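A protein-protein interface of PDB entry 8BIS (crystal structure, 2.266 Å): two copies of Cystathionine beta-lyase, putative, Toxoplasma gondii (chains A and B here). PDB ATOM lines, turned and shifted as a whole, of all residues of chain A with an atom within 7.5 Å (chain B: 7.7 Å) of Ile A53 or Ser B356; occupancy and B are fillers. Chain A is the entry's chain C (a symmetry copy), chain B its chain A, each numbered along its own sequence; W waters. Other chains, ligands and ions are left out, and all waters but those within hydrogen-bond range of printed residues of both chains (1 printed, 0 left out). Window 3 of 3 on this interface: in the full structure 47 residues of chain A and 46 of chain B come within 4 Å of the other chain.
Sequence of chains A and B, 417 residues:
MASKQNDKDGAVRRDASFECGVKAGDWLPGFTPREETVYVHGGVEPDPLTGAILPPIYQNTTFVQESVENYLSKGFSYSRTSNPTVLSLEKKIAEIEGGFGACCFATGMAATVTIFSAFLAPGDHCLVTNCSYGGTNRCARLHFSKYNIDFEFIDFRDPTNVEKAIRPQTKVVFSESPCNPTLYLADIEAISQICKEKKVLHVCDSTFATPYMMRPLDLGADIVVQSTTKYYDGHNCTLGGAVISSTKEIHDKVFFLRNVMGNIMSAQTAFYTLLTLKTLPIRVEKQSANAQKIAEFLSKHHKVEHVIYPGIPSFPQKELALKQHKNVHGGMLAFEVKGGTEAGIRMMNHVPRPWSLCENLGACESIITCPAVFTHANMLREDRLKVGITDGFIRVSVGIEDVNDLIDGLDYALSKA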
ATOM      1  N   ALA A  24      13.547 -10.160 -13.982  1.00  0.00           N
ATOM      2  CA  ALA A  24      13.999 -10.150 -15.366  1.00  0.00           C
ATOM      3  C   ALA A  24      12.930  -9.548 -16.267  1.00  0.00           C
ATOM      4  O   ALA A  24      11.753  -9.909 -16.183  1.00  0.00           O
ATOM      5  CB  ALA A  24      14.341 -11.570 -15.820  1.00  0.00           C
ATOM      6  N   GLY A  25      13.344  -8.624 -17.132  1.00  0.00           N
ATOM      7  CA  GLY A  25      12.439  -7.872 -17.966  1.00  0.00           C
ATOM      8  C   GLY A  25      12.184  -6.457 -17.491  1.00  0.00           C
ATOM      9  O   GLY A  25      11.677  -5.639 -18.265  1.00  0.00           O
ATOM     10  N   HIS A  41      18.821  -0.619 -26.903  1.00  0.00           N
ATOM     11  CA  HIS A  41      17.521  -1.058 -26.412  1.00  0.00           C
ATOM     12  C   HIS A  41      16.446   0.017 -26.371  1.00  0.00           C
ATOM     13  O   HIS A  41      15.266  -0.334 -26.242  1.00  0.00           O
ATOM     14  CB  HIS A  41      17.654  -1.638 -24.995  1.00  0.00           C
ATOM     15  CG  HIS A  41      18.577  -2.810 -24.904  1.00  0.00           C
ATOM     16  ND1 HIS A  41      18.209  -4.080 -25.292  1.00  0.00           N
ATOM     17  CD2 HIS A  41      19.851  -2.908 -24.460  1.00  0.00           C
ATOM     18  CE1 HIS A  41      19.219  -4.908 -25.093  1.00  0.00           C
ATOM     19  NE2 HIS A  41      20.226  -4.223 -24.585  1.00  0.00           N
ATOM     20  N   VAL A  44      12.440   0.061 -27.260  1.00  0.00           N
ATOM     21  CA  VAL A  44      12.110  -1.300 -27.669  1.00  0.00           C
ATOM     22  C   VAL A  44      12.208  -2.214 -26.457  1.00  0.00           C
ATOM     23  O   VAL A  44      13.221  -2.210 -25.750  1.00  0.00           O
ATOM     24  CB  VAL A  44      13.032  -1.806 -28.795  1.00  0.00           C
ATOM     25  CG1 VAL A  44      12.870  -3.311 -28.983  1.00  0.00           C
ATOM     26  CG2 VAL A  44      12.741  -1.071 -30.093  1.00  0.00           C
ATOM     27  N   GLU A  45      11.157  -2.984 -26.216  1.00  0.00           N
ATOM     28  CA  GLU A  45      11.121  -4.055 -25.238  1.00  0.00           C
ATOM     29  C   GLU A  45      10.714  -5.341 -25.945  1.00  0.00           C
ATOM     30  O   GLU A  45      10.177  -5.298 -27.059  1.00  0.00           O
ATOM     31  CB  GLU A  45      10.132  -3.737 -24.106  1.00  0.00           C
ATOM     32  CG  GLU A  45      10.561  -2.578 -23.212  1.00  0.00           C
ATOM     33  CD  GLU A  45      11.681  -2.950 -22.253  1.00  0.00           C
ATOM     34  OE1 GLU A  45      11.376  -3.435 -21.143  1.00  0.00           O
ATOM     35  OE2 GLU A  45      12.864  -2.753 -22.604  1.00  0.00           O
ATOM     36  N   PRO A  46      10.975  -6.505 -25.346  1.00  0.00           N
ATOM     37  CA  PRO A  46      10.518  -7.756 -25.953  1.00  0.00           C
ATOM     38  C   PRO A  46       9.021  -7.714 -26.226  1.00  0.00           C
ATOM     39  O   PRO A  46       8.261  -7.042 -25.524  1.00  0.00           O
ATOM     40  CB  PRO A  46      10.871  -8.813 -24.899  1.00  0.00           C
ATOM     41  CG  PRO A  46      12.036  -8.229 -24.173  1.00  0.00           C
ATOM     42  CD  PRO A  46      11.782  -6.744 -24.133  1.00  0.00           C
ATOM     43  N   ASP A  47       8.611  -8.416 -27.274  1.00  0.00           N
ATOM     44  CA  ASP A  47       7.205  -8.454 -27.638  1.00  0.00           C
ATOM     45  C   ASP A  47       6.392  -8.990 -26.463  1.00  0.00           C
ATOM     46  O   ASP A  47       6.726 -10.050 -25.918  1.00  0.00           O
ATOM     47  CB  ASP A  47       6.998  -9.324 -28.876  1.00  0.00           C
ATOM     48  CG  ASP A  47       5.538  -9.654 -29.125  1.00  0.00           C
ATOM     49  OD1 ASP A  47       4.703  -8.720 -29.158  1.00  0.00           O
ATOM     50  OD2 ASP A  47       5.228 -10.852 -29.302  1.00  0.00           O
ATOM     51  N   THR A  50       4.933 -12.705 -27.407  1.00  0.00           N
ATOM     52  CA  THR A  50       5.813 -13.853 -27.565  1.00  0.00           C
ATOM     53  C   THR A  50       7.151 -13.730 -26.852  1.00  0.00           C
ATOM     54  O   THR A  50       7.894 -14.717 -26.800  1.00  0.00           O
ATOM     55  CB  THR A  50       6.088 -14.111 -29.055  1.00  0.00           C
ATOM     56  OG1 THR A  50       6.824 -13.009 -29.596  1.00  0.00           O
ATOM     57  CG2 THR A  50       4.789 -14.254 -29.817  1.00  0.00           C
ATOM     58  N   GLY A  51       7.488 -12.565 -26.308  1.00  0.00           N
ATOM     59  CA  GLY A  51       8.824 -12.354 -25.793  1.00  0.00           C
ATOM     60  C   GLY A  51       9.874 -12.143 -26.856  1.00  0.00           C
ATOM     61  O   GLY A  51      11.063 -12.074 -26.523  1.00  0.00           O
ATOM     62  N   ALA A  52       9.472 -12.049 -28.124  1.00  0.00           N
ATOM     63  CA  ALA A  52      10.417 -11.848 -29.213  1.00  0.00           C
ATOM     64  C   ALA A  52      11.321 -10.664 -28.915  1.00  0.00           C
ATOM     65  O   ALA A  52      10.850  -9.564 -28.613  1.00  0.00           O
ATOM     66  CB  ALA A  52       9.670 -11.633 -30.530  1.00  0.00           C
ATOM     67  N   ILE A  53      12.628 -10.908 -28.987  1.00  0.00           N
ATOM     68  CA  ILE A  53      13.590  -9.906 -28.546  1.00  0.00           C
ATOM     69  C   ILE A  53      13.593  -8.706 -29.482  1.00  0.00           C
ATOM     70  O   ILE A  53      13.876  -7.580 -29.057  1.00  0.00           O
ATOM     71  CB  ILE A  53      14.981 -10.549 -28.418  1.00  0.00           C
ATOM     72  CG1 ILE A  53      15.904  -9.670 -27.580  1.00  0.00           C
ATOM     73  CG2 ILE A  53      15.569 -10.831 -29.795  1.00  0.00           C
ATOM     74  CD1 ILE A  53      17.118 -10.406 -27.043  1.00  0.00           C
ATOM     75  N   LEU A  54      13.274  -8.911 -30.747  1.00  0.00           N
ATOM     76  CA  LEU A  54      13.187  -7.816 -31.690  1.00  0.00           C
ATOM     77  C   LEU A  54      11.730  -7.488 -31.985  1.00  0.00           C
ATOM     78  O   LEU A  54      10.862  -8.361 -31.891  1.00  0.00           O
ATOM     79  CB  LEU A  54      13.905  -8.160 -32.999  1.00  0.00           C
ATOM     80  CG  LEU A  54      15.419  -8.362 -32.924  1.00  0.00           C
ATOM     81  CD1 LEU A  54      16.007  -8.421 -34.324  1.00  0.00           C
ATOM     82  CD2 LEU A  54      16.073  -7.264 -32.097  1.00  0.00           C
ATOM     83  N   PRO A  55      11.433  -6.243 -32.340  1.00  0.00           N
ATOM     84  CA  PRO A  55      10.060  -5.881 -32.692  1.00  0.00           C
ATOM     85  C   PRO A  55       9.616  -6.608 -33.947  1.00  0.00           C
ATOM     86  O   PRO A  55      10.322  -6.588 -34.968  1.00  0.00           O
ATOM     87  CB  PRO A  55      10.142  -4.366 -32.930  1.00  0.00           C
ATOM     88  CG  PRO A  55      11.572  -4.128 -33.306  1.00  0.00           C
ATOM     89  CD  PRO A  55      12.356  -5.101 -32.474  1.00  0.00           C
ATOM     90  N   PRO A  56       8.460  -7.269 -33.911  1.00  0.00           N
ATOM     91  CA  PRO A  56       7.933  -7.880 -35.133  1.00  0.00           C
ATOM     92  C   PRO A  56       7.617  -6.816 -36.168  1.00  0.00           C
ATOM     93  O   PRO A  56       7.249  -5.687 -35.837  1.00  0.00           O
ATOM     94  CB  PRO A  56       6.665  -8.602 -34.657  1.00  0.00           C
ATOM     95  CG  PRO A  56       6.304  -7.948 -33.377  1.00  0.00           C
ATOM     96  CD  PRO A  56       7.596  -7.519 -32.748  1.00  0.00           C
ATOM     97  N   LYS A 278      21.429   0.461 -33.556  1.00  0.00           N
ATOM     98  CA  LYS A 278      22.093  -0.142 -32.406  1.00  0.00           C
ATOM     99  C   LYS A 278      23.603   0.029 -32.470  1.00  0.00           C
ATOM    100  O   LYS A 278      24.255   0.167 -31.429  1.00  0.00           O
ATOM    101  CB  LYS A 278      21.717  -1.623 -32.313  1.00  0.00           C
ATOM    102  CG  LYS A 278      20.211  -1.853 -32.198  1.00  0.00           C
ATOM    103  CD  LYS A 278      19.859  -3.295 -31.862  1.00  0.00           C
ATOM    104  CE  LYS A 278      20.291  -4.256 -32.958  1.00  0.00           C
ATOM    105  NZ  LYS A 278      19.705  -5.618 -32.762  1.00  0.00           N
ATOM    106  N   HIS B 235      22.625  -9.324 -34.461  1.00  0.00           N
ATOM    107  CA  HIS B 235      21.489  -8.445 -34.202  1.00  0.00           C
ATOM    108  C   HIS B 235      20.228  -9.209 -33.816  1.00  0.00           C
ATOM    109  O   HIS B 235      19.147  -8.609 -33.789  1.00  0.00           O
ATOM    110  CB  HIS B 235      21.189  -7.565 -35.419  1.00  0.00           C
ATOM    111  CG  HIS B 235      22.262  -6.569 -35.734  1.00  0.00           C
ATOM    112  ND1 HIS B 235      23.459  -6.924 -36.319  1.00  0.00           N
ATOM    113  CD2 HIS B 235      22.311  -5.227 -35.562  1.00  0.00           C
ATOM    114  CE1 HIS B 235      24.202  -5.846 -36.489  1.00  0.00           C
ATOM    115  NE2 HIS B 235      23.529  -4.802 -36.037  1.00  0.00           N
ATOM    116  N   ASN B 236      20.336 -10.509 -33.523  1.00  0.00           N
ATOM    117  CA  ASN B 236      19.190 -11.348 -33.163  1.00  0.00           C
ATOM    118  C   ASN B 236      18.142 -11.380 -34.267  1.00  0.00           C
ATOM    119  O   ASN B 236      16.960 -11.606 -34.008  1.00  0.00           O
ATOM    120  CB  ASN B 236      18.550 -10.897 -31.846  1.00  0.00           C
ATOM    121  CG  ASN B 236      19.283 -11.422 -30.633  1.00  0.00           C
ATOM    122  OD1 ASN B 236      19.543 -12.619 -30.525  1.00  0.00           O
ATOM    123  ND2 ASN B 236      19.627 -10.529 -29.714  1.00  0.00           N
ATOM    124  N   CYS B 237      18.572 -11.183 -35.510  1.00  0.00           N
ATOM    125  CA  CYS B 237      17.652 -10.949 -36.613  1.00  0.00           C
ATOM    126  C   CYS B 237      17.363 -12.199 -37.436  1.00  0.00           C
ATOM    127  O   CYS B 237      16.196 -12.530 -37.668  1.00  0.00           O
ATOM    128  CB  CYS B 237      18.213  -9.844 -37.514  1.00  0.00           C
ATOM    129  SG  CYS B 237      17.151  -9.412 -38.882  1.00  0.00           S
ATOM    130  N   MET B 348      19.098 -15.713 -12.192  1.00  0.00           N
ATOM    131  CA  MET B 348      18.515 -15.623 -13.527  1.00  0.00           C
ATOM    132  C   MET B 348      17.175 -14.905 -13.500  1.00  0.00           C
ATOM    133  O   MET B 348      16.893 -14.065 -14.361  1.00  0.00           O
ATOM    134  CB  MET B 348      18.345 -17.020 -14.123  1.00  0.00           C
ATOM    135  CG  MET B 348      19.641 -17.772 -14.360  1.00  0.00           C
ATOM    136  SD  MET B 348      20.383 -17.433 -15.957  1.00  0.00           S
ATOM    137  CE  MET B 348      21.364 -15.993 -15.575  1.00  0.00           C
ATOM    138  N   VAL B 351      17.868 -10.898 -13.065  1.00  0.00           N
ATOM    139  CA  VAL B 351      18.800 -10.138 -13.886  1.00  0.00           C
ATOM    140  C   VAL B 351      17.986  -9.107 -14.684  1.00  0.00           C
ATOM    141  O   VAL B 351      17.102  -9.511 -15.452  1.00  0.00           O
ATOM    142  CB  VAL B 351      19.637 -11.036 -14.802  1.00  0.00           C
ATOM    143  CG1 VAL B 351      18.771 -11.898 -15.718  1.00  0.00           C
ATOM    144  CG2 VAL B 351      20.625 -10.205 -15.605  1.00  0.00           C
ATOM    145  N   PRO B 352      18.213  -7.820 -14.487  1.00  0.00           N
ATOM    146  CA  PRO B 352      17.331  -6.812 -15.080  1.00  0.00           C
ATOM    147  C   PRO B 352      17.811  -6.384 -16.462  1.00  0.00           C
ATOM    148  O   PRO B 352      18.889  -6.762 -16.922  1.00  0.00           O
ATOM    149  CB  PRO B 352      17.435  -5.653 -14.081  1.00  0.00           C
ATOM    150  CG  PRO B 352      18.841  -5.746 -13.587  1.00  0.00           C
ATOM    151  CD  PRO B 352      19.219  -7.213 -13.601  1.00  0.00           C
ATOM    152  N   ARG B 353      16.976  -5.583 -17.118  1.00  0.00           N
ATOM    153  CA  ARG B 353      17.373  -4.969 -18.373  1.00  0.00           C
ATOM    154  C   ARG B 353      18.576  -4.056 -18.130  1.00  0.00           C
ATOM    155  O   ARG B 353      18.756  -3.540 -17.022  1.00  0.00           O
ATOM    156  CB  ARG B 353      16.211  -4.181 -18.968  1.00  0.00           C
ATOM    157  CG  ARG B 353      14.878  -4.886 -18.870  1.00  0.00           C
ATOM    158  CD  ARG B 353      14.566  -5.631 -20.145  1.00  0.00           C
ATOM    159  NE  ARG B 353      14.398  -4.710 -21.263  1.00  0.00           N
ATOM    160  CZ  ARG B 353      15.152  -4.717 -22.356  1.00  0.00           C
ATOM    161  NH1 ARG B 353      16.126  -5.608 -22.485  1.00  0.00           N
ATOM    162  NH2 ARG B 353      14.926  -3.835 -23.323  1.00  0.00           N
ATOM    163  N   PRO B 354      19.422  -3.827 -19.150  1.00  0.00           N
ATOM    164  CA  PRO B 354      19.319  -4.203 -20.566  1.00  0.00           C
ATOM    165  C   PRO B 354      19.562  -5.684 -20.880  1.00  0.00           C
ATOM    166  O   PRO B 354      19.518  -6.054 -22.052  1.00  0.00           O
ATOM    167  CB  PRO B 354      20.404  -3.349 -21.220  1.00  0.00           C
ATOM    168  CG  PRO B 354      21.429  -3.198 -20.169  1.00  0.00           C
ATOM    169  CD  PRO B 354      20.673  -3.099 -18.872  1.00  0.00           C
ATOM    170  N   TRP B 355      19.810  -6.509 -19.866  1.00  0.00           N
ATOM    171  CA  TRP B 355      19.987  -7.936 -20.100  1.00  0.00           C
ATOM    172  C   TRP B 355      18.688  -8.571 -20.573  1.00  0.00           C
ATOM    173  O   TRP B 355      17.588  -8.102 -20.270  1.00  0.00           O
ATOM    174  CB  TRP B 355      20.456  -8.646 -18.832  1.00  0.00           C
ATOM    175  CG  TRP B 355      21.834  -8.283 -18.401  1.00  0.00           C
ATOM    176  CD1 TRP B 355      22.182  -7.335 -17.481  1.00  0.00           C
ATOM    177  CD2 TRP B 355      23.055  -8.862 -18.867  1.00  0.00           C
ATOM    178  NE1 TRP B 355      23.549  -7.288 -17.347  1.00  0.00           N
ATOM    179  CE2 TRP B 355      24.108  -8.215 -18.189  1.00  0.00           C
ATOM    180  CE3 TRP B 355      23.363  -9.860 -19.794  1.00  0.00           C
ATOM    181  CZ2 TRP B 355      25.445  -8.537 -18.409  1.00  0.00           C
ATOM    182  CZ3 TRP B 355      24.691 -10.177 -20.013  1.00  0.00           C
ATOM    183  CH2 TRP B 355      25.715  -9.518 -19.324  1.00  0.00           C
ATOM    184  N   SER B 356      18.826  -9.665 -21.315  1.00  0.00           N
ATOM    185  CA  SER B 356      17.686 -10.443 -21.774  1.00  0.00           C
ATOM    186  C   SER B 356      17.921 -11.903 -21.425  1.00  0.00           C
ATOM    187  O   SER B 356      18.941 -12.480 -21.817  1.00  0.00           O
ATOM    188  CB  SER B 356      17.466 -10.273 -23.280  1.00  0.00           C
ATOM    189  OG  SER B 356      17.319  -8.907 -23.619  1.00  0.00           O
ATOM    190  N   LEU B 357      16.987 -12.488 -20.681  1.00  0.00           N
ATOM    191  CA  LEU B 357      17.022 -13.909 -20.361  1.00  0.00           C
ATOM    192  C   LEU B 357      16.422 -14.676 -21.533  1.00  0.00           C
ATOM    193  O   LEU B 357      15.200 -14.664 -21.733  1.00  0.00           O
ATOM    194  CB  LEU B 357      16.259 -14.181 -19.069  1.00  0.00           C
ATOM    195  CG  LEU B 357      16.324 -15.603 -18.509  1.00  0.00           C
ATOM    196  CD1 LEU B 357      17.748 -15.967 -18.130  1.00  0.00           C
ATOM    197  CD2 LEU B 357      15.400 -15.730 -17.314  1.00  0.00           C
ATOM    198  N   CYS B 358      17.277 -15.336 -22.309  1.00  0.00           N
ATOM    199  CA  CYS B 358      16.870 -15.990 -23.548  1.00  0.00           C
ATOM    200  C   CYS B 358      18.025 -16.858 -24.034  1.00  0.00           C
ATOM    201  O   CYS B 358      19.068 -16.956 -23.380  1.00  0.00           O
ATOM    202  CB  CYS B 358      16.448 -14.954 -24.593  1.00  0.00           C
ATOM    203  SG  CYS B 358      17.782 -13.873 -25.137  1.00  0.00           S
ATOM    204  N   GLU B 359      17.827 -17.500 -25.182  1.00  0.00           N
ATOM    205  CA  GLU B 359      18.887 -18.264 -25.826  1.00  0.00           C
ATOM    206  C   GLU B 359      19.576 -17.367 -26.857  1.00  0.00           C
ATOM    207  O   GLU B 359      19.471 -16.141 -26.783  1.00  0.00           O
ATOM    208  CB  GLU B 359      18.316 -19.562 -26.409  1.00  0.00           C
ATOM    209  CG  GLU B 359      17.872 -20.551 -25.330  1.00  0.00           C
ATOM    210  CD  GLU B 359      16.739 -21.462 -25.774  1.00  0.00           C
ATOM    211  OE1 GLU B 359      16.801 -21.988 -26.907  1.00  0.00           O
ATOM    212  OE2 GLU B 359      15.786 -21.653 -24.988  1.00  0.00           O
ATOM    213  N   ASN B 360      20.300 -17.963 -27.809  1.00  0.00           N
ATOM    214  CA  ASN B 360      21.115 -17.237 -28.782  1.00  0.00           C
ATOM    215  C   ASN B 360      22.276 -16.514 -28.097  1.00  0.00           C
ATOM    216  O   ASN B 360      22.326 -16.433 -26.865  1.00  0.00           O
ATOM    217  CB  ASN B 360      20.259 -16.252 -29.588  1.00  0.00           C
ATOM    218  CG  ASN B 360      20.919 -15.829 -30.882  1.00  0.00           C
ATOM    219  OD1 ASN B 360      21.664 -16.594 -31.484  1.00  0.00           O
ATOM    220  ND2 ASN B 360      20.645 -14.603 -31.320  1.00  0.00           N
ATOM    221  N   ALA B 363      25.046 -11.250 -29.995  1.00  0.00           N
ATOM    222  CA  ALA B 363      24.276 -10.135 -30.526  1.00  0.00           C
ATOM    223  C   ALA B 363      24.613  -8.825 -29.819  1.00  0.00           C
ATOM    224  O   ALA B 363      25.272  -8.792 -28.776  1.00  0.00           O
ATOM    225  CB  ALA B 363      22.776 -10.420 -30.414  1.00  0.00           C
ATOM    226  N   GLU B 365      22.510  -7.106 -28.290  1.00  0.00           N
ATOM    227  CA  GLU B 365      21.806  -7.189 -27.022  1.00  0.00           C
ATOM    228  C   GLU B 365      22.468  -8.241 -26.140  1.00  0.00           C
ATOM    229  O   GLU B 365      22.634  -9.393 -26.554  1.00  0.00           O
ATOM    230  CB  GLU B 365      20.339  -7.545 -27.254  1.00  0.00           C
ATOM    231  CG  GLU B 365      19.559  -6.595 -28.159  1.00  0.00           C
ATOM    232  CD  GLU B 365      19.776  -6.864 -29.639  1.00  0.00           C
ATOM    233  OE1 GLU B 365      20.492  -7.829 -29.978  1.00  0.00           O
ATOM    234  OE2 GLU B 365      19.223  -6.106 -30.464  1.00  0.00           O
ATOM    235  N   SER B 366      22.839  -7.847 -24.926  1.00  0.00           N
ATOM    236  CA  SER B 366      23.477  -8.777 -24.005  1.00  0.00           C
ATOM    237  C   SER B 366      22.489  -9.844 -23.555  1.00  0.00           C
ATOM    238  O   SER B 366      21.348  -9.542 -23.193  1.00  0.00           O
ATOM    239  CB  SER B 366      24.039  -8.031 -22.801  1.00  0.00           C
ATOM    240  OG  SER B 366      25.061  -7.141 -23.204  1.00  0.00           O
ATOM    241  N   ILE B 367      22.939 -11.095 -23.574  1.00  0.00           N
ATOM    242  CA  ILE B 367      22.105 -12.256 -23.301  1.00  0.00           C
ATOM    243  C   ILE B 367      22.753 -13.061 -22.185  1.00  0.00           C
ATOM    244  O   ILE B 367      23.980 -13.192 -22.133  1.00  0.00           O
ATOM    245  CB  ILE B 367      21.925 -13.114 -24.570  1.00  0.00           C
ATOM    246  CG1 ILE B 367      21.106 -12.353 -25.612  1.00  0.00           C
ATOM    247  CG2 ILE B 367      21.264 -14.440 -24.246  1.00  0.00           C
ATOM    248  CD1 ILE B 367      21.084 -13.014 -26.972  1.00  0.00           C
ATOM    249  N   ILE B 368      21.933 -13.588 -21.285  1.00  0.00           N
ATOM    250  CA  ILE B 368      22.419 -14.422 -20.196  1.00  0.00           C
ATOM    251  C   ILE B 368      21.548 -15.669 -20.110  1.00  0.00           C
ATOM    252  O   ILE B 368      20.328 -15.602 -20.307  1.00  0.00           O
ATOM    253  CB  ILE B 368      22.448 -13.643 -18.861  1.00  0.00           C
ATOM    254  CG1 ILE B 368      23.470 -14.262 -17.909  1.00  0.00           C
ATOM    255  CG2 ILE B 368      21.067 -13.566 -18.229  1.00  0.00           C
ATOM    256  CD1 ILE B 368      23.799 -13.388 -16.719  1.00  0.00           C
ATOM    257  N   THR B 369      22.179 -16.813 -19.850  1.00  0.00           N
ATOM    258  CA  THR B 369      21.447 -18.068 -19.759  1.00  0.00           C
ATOM    259  C   THR B 369      22.123 -18.985 -18.750  1.00  0.00           C
ATOM    260  O   THR B 369      23.310 -18.845 -18.446  1.00  0.00           O
ATOM    261  CB  THR B 369      21.352 -18.771 -21.118  1.00  0.00           C
ATOM    262  OG1 THR B 369      20.506 -19.922 -21.002  1.00  0.00           O
ATOM    263  CG2 THR B 369      22.730 -19.205 -21.596  1.00  0.00           C
ATOM    264  N   ARG B 395      26.171 -18.954 -18.803  1.00  0.00           N
ATOM    265  CA  ARG B 395      26.770 -18.475 -20.038  1.00  0.00           C
ATOM    266  C   ARG B 395      26.303 -17.050 -20.305  1.00  0.00           C
ATOM    267  O   ARG B 395      25.113 -16.737 -20.168  1.00  0.00           O
ATOM    268  CB  ARG B 395      26.393 -19.381 -21.212  1.00  0.00           C
ATOM    269  CG  ARG B 395      27.059 -19.012 -22.528  1.00  0.00           C
ATOM    270  CD  ARG B 395      26.526 -19.859 -23.681  1.00  0.00           C
ATOM    271  NE  ARG B 395      25.190 -19.450 -24.114  1.00  0.00           N
ATOM    272  CZ  ARG B 395      24.439 -20.136 -24.972  1.00  0.00           C
ATOM    273  NH1 ARG B 395      24.891 -21.269 -25.490  1.00  0.00           N
ATOM    274  NH2 ARG B 395      23.237 -19.694 -25.314  1.00  0.00           N
ATOM    275  N   SER B 397      26.599 -13.862 -23.067  1.00  0.00           N
ATOM    276  CA  SER B 397      26.935 -13.210 -24.323  1.00  0.00           C
ATOM    277  C   SER B 397      26.888 -11.708 -24.091  1.00  0.00           C
ATOM    278  O   SER B 397      25.832 -11.162 -23.753  1.00  0.00           O
ATOM    279  CB  SER B 397      25.961 -13.611 -25.428  1.00  0.00           C
ATOM    280  OG  SER B 397      26.359 -13.068 -26.671  1.00  0.00           O
ATOM    281  N   GLU B 401      25.984  -2.676 -25.290  1.00  0.00           N
ATOM    282  CA  GLU B 401      25.457  -1.644 -24.405  1.00  0.00           C
ATOM    283  C   GLU B 401      26.580  -1.020 -23.589  1.00  0.00           C
ATOM    284  O   GLU B 401      27.739  -1.439 -23.677  1.00  0.00           O
ATOM    285  CB  GLU B 401      24.389  -2.205 -23.461  1.00  0.00           C
ATOM    286  CG  GLU B 401      23.231  -2.905 -24.148  1.00  0.00           C
ATOM    287  CD  GLU B 401      23.454  -4.400 -24.278  1.00  0.00           C
ATOM    288  OE1 GLU B 401      24.627  -4.819 -24.265  1.00  0.00           O
ATOM    289  OE2 GLU B 401      22.460  -5.152 -24.395  1.00  0.00           O
ATOM    290  N   LEU B 406      25.438  -3.015 -17.795  1.00  0.00           N
ATOM    291  CA  LEU B 406      25.530  -4.468 -17.699  1.00  0.00           C
ATOM    292  C   LEU B 406      26.102  -4.899 -16.355  1.00  0.00           C
ATOM    293  O   LEU B 406      25.607  -5.852 -15.739  1.00  0.00           O
ATOM    294  CB  LEU B 406      26.380  -5.005 -18.849  1.00  0.00           C
ATOM    295  CG  LEU B 406      25.869  -4.628 -20.242  1.00  0.00           C
ATOM    296  CD1 LEU B 406      26.865  -5.011 -21.325  1.00  0.00           C
ATOM    297  CD2 LEU B 406      24.507  -5.267 -20.498  1.00  0.00           C
HETATM  298  O   HOH W   1      16.099  -8.876 -18.099  1.00  0.00           O
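No position is printed for both chains. Of the 17 pairs that touch across the chains among the printed residues, none has its exchanged pair printed and touching as well.
Printed residues of chain B within 4 Å of Ile A53: Asn B236 and Ser B356. Of the printed residues of chain A, His B235 touches Leu A54 (3.2 Å) and Lys A278 (3.2 Å). Of the printed residues of chain A, Met B348 touches Ala A24 (3.9 Å). Printed residues of chain A within 4 Å of Arg B353: Gly A25 (3.3 Å), His A41 (3.8 Å), Val A44 (3.4 Å) and Glu A45 (2.4 Å). Of the printed residues of chain A, Pro B354 touches His A41 (3.2 Å). Of the printed residues of chain A, Glu B365 touches His A41, Leu A54 and Lys A278.
Of the 24 printed residues of chain B, 10 touch a printed residue of chain A. Printed residues of chain B that touch a printed residue of chain A: His B235, Asn B236, Cys B237, Met B348, Val B351, Arg B353, Pro B354, Ser B356, Glu B365 and Glu B401. Hydrophobic or aromatic side chains of chain B within 4 Å of the printed part of chain A: His B235 and Pro B354. Hydrophobic or aromatic side chains of chain A that line the printed part of chain B: Ala A24, His A41, Ile A53 and Leu A54. Among the printed residues, Asp or Glu carboxylates within 4 Å of a Lys or Arg side-chain nitrogen of the other chain: Glu A45 with Arg B353 (2.4 Å) and Lys A278 with Glu B365 (2.4 Å).
Met B348 touches Ala A24. Val B351 touches Ala A24. Arg B353 touches Gly A25. ND1 of His A41 touches NH1 of Arg B353, 3.8 Å away. His A41 touches Glu B365 (CE1 to CG, 3.5 Å). Ile A53 touches Asn B236 (CG2 to CB, 3.6 Å). Ile A53 touches Ser B356 (CD1 to OG, 3.7 Å). Leu A54 touches His B235. Leu A54 touches Asn B236. CD2 of Leu A54 touches OE2 of Glu B365, at 3.7 Å.
Water W1 lies within hydrogen-bond range of O of Trp B355, O of Val B351 and N of Gly A25.
OE2 of Glu B401 lies within hydrogen-bond range of NE2 of His A41 (2.4 Å). NH2 of Arg B353 is in salt-bridge range of OE2 of Glu A45, 2.4 Å away. The backbone carbonyl oxygen (O) of Val A44 is in hydrogen-bond range of the guanidinium group (NH2) of Arg B353 (3.4 Å). The backbone carbonyl oxygen of Pro B354 lies within hydrogen-bond range of a ring nitrogen (NE2) of His A41. The backbone carbonyl oxygen (O) of His B235 is in hydrogen-bond range of the side-chain amino group (NZ) of Lys A278, at 3.2 Å. The side-chain carboxylate of Glu B365 lies within salt-bridge range of the side-chain amino group of Lys A278 (3.6 Å).
ND2 of Asn B236 lies within hydrogen-bond range of OE1 of Glu B365, at 2.8 Å. OD1 of Asn B236 is in hydrogen-bond range of ND2 of Asn B360 (2.4 Å). The backbone NH of Ser B356 sits at hydrogen-bond distance from the backbone carbonyl oxygen of Ser B366 (3.1 Å). O of Ser B356 sits at hydrogen-bond distance from SG of Cys B358 (3.8 Å). N of Ile B368 sits at hydrogen-bond distance from O of Ser B356, at 3.2 Å. The side-chain hydroxyl (OG) of Ser B366 sits at hydrogen-bond distance from the side-chain carboxylate (OE1) of Glu B401, at 2.6 Å.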
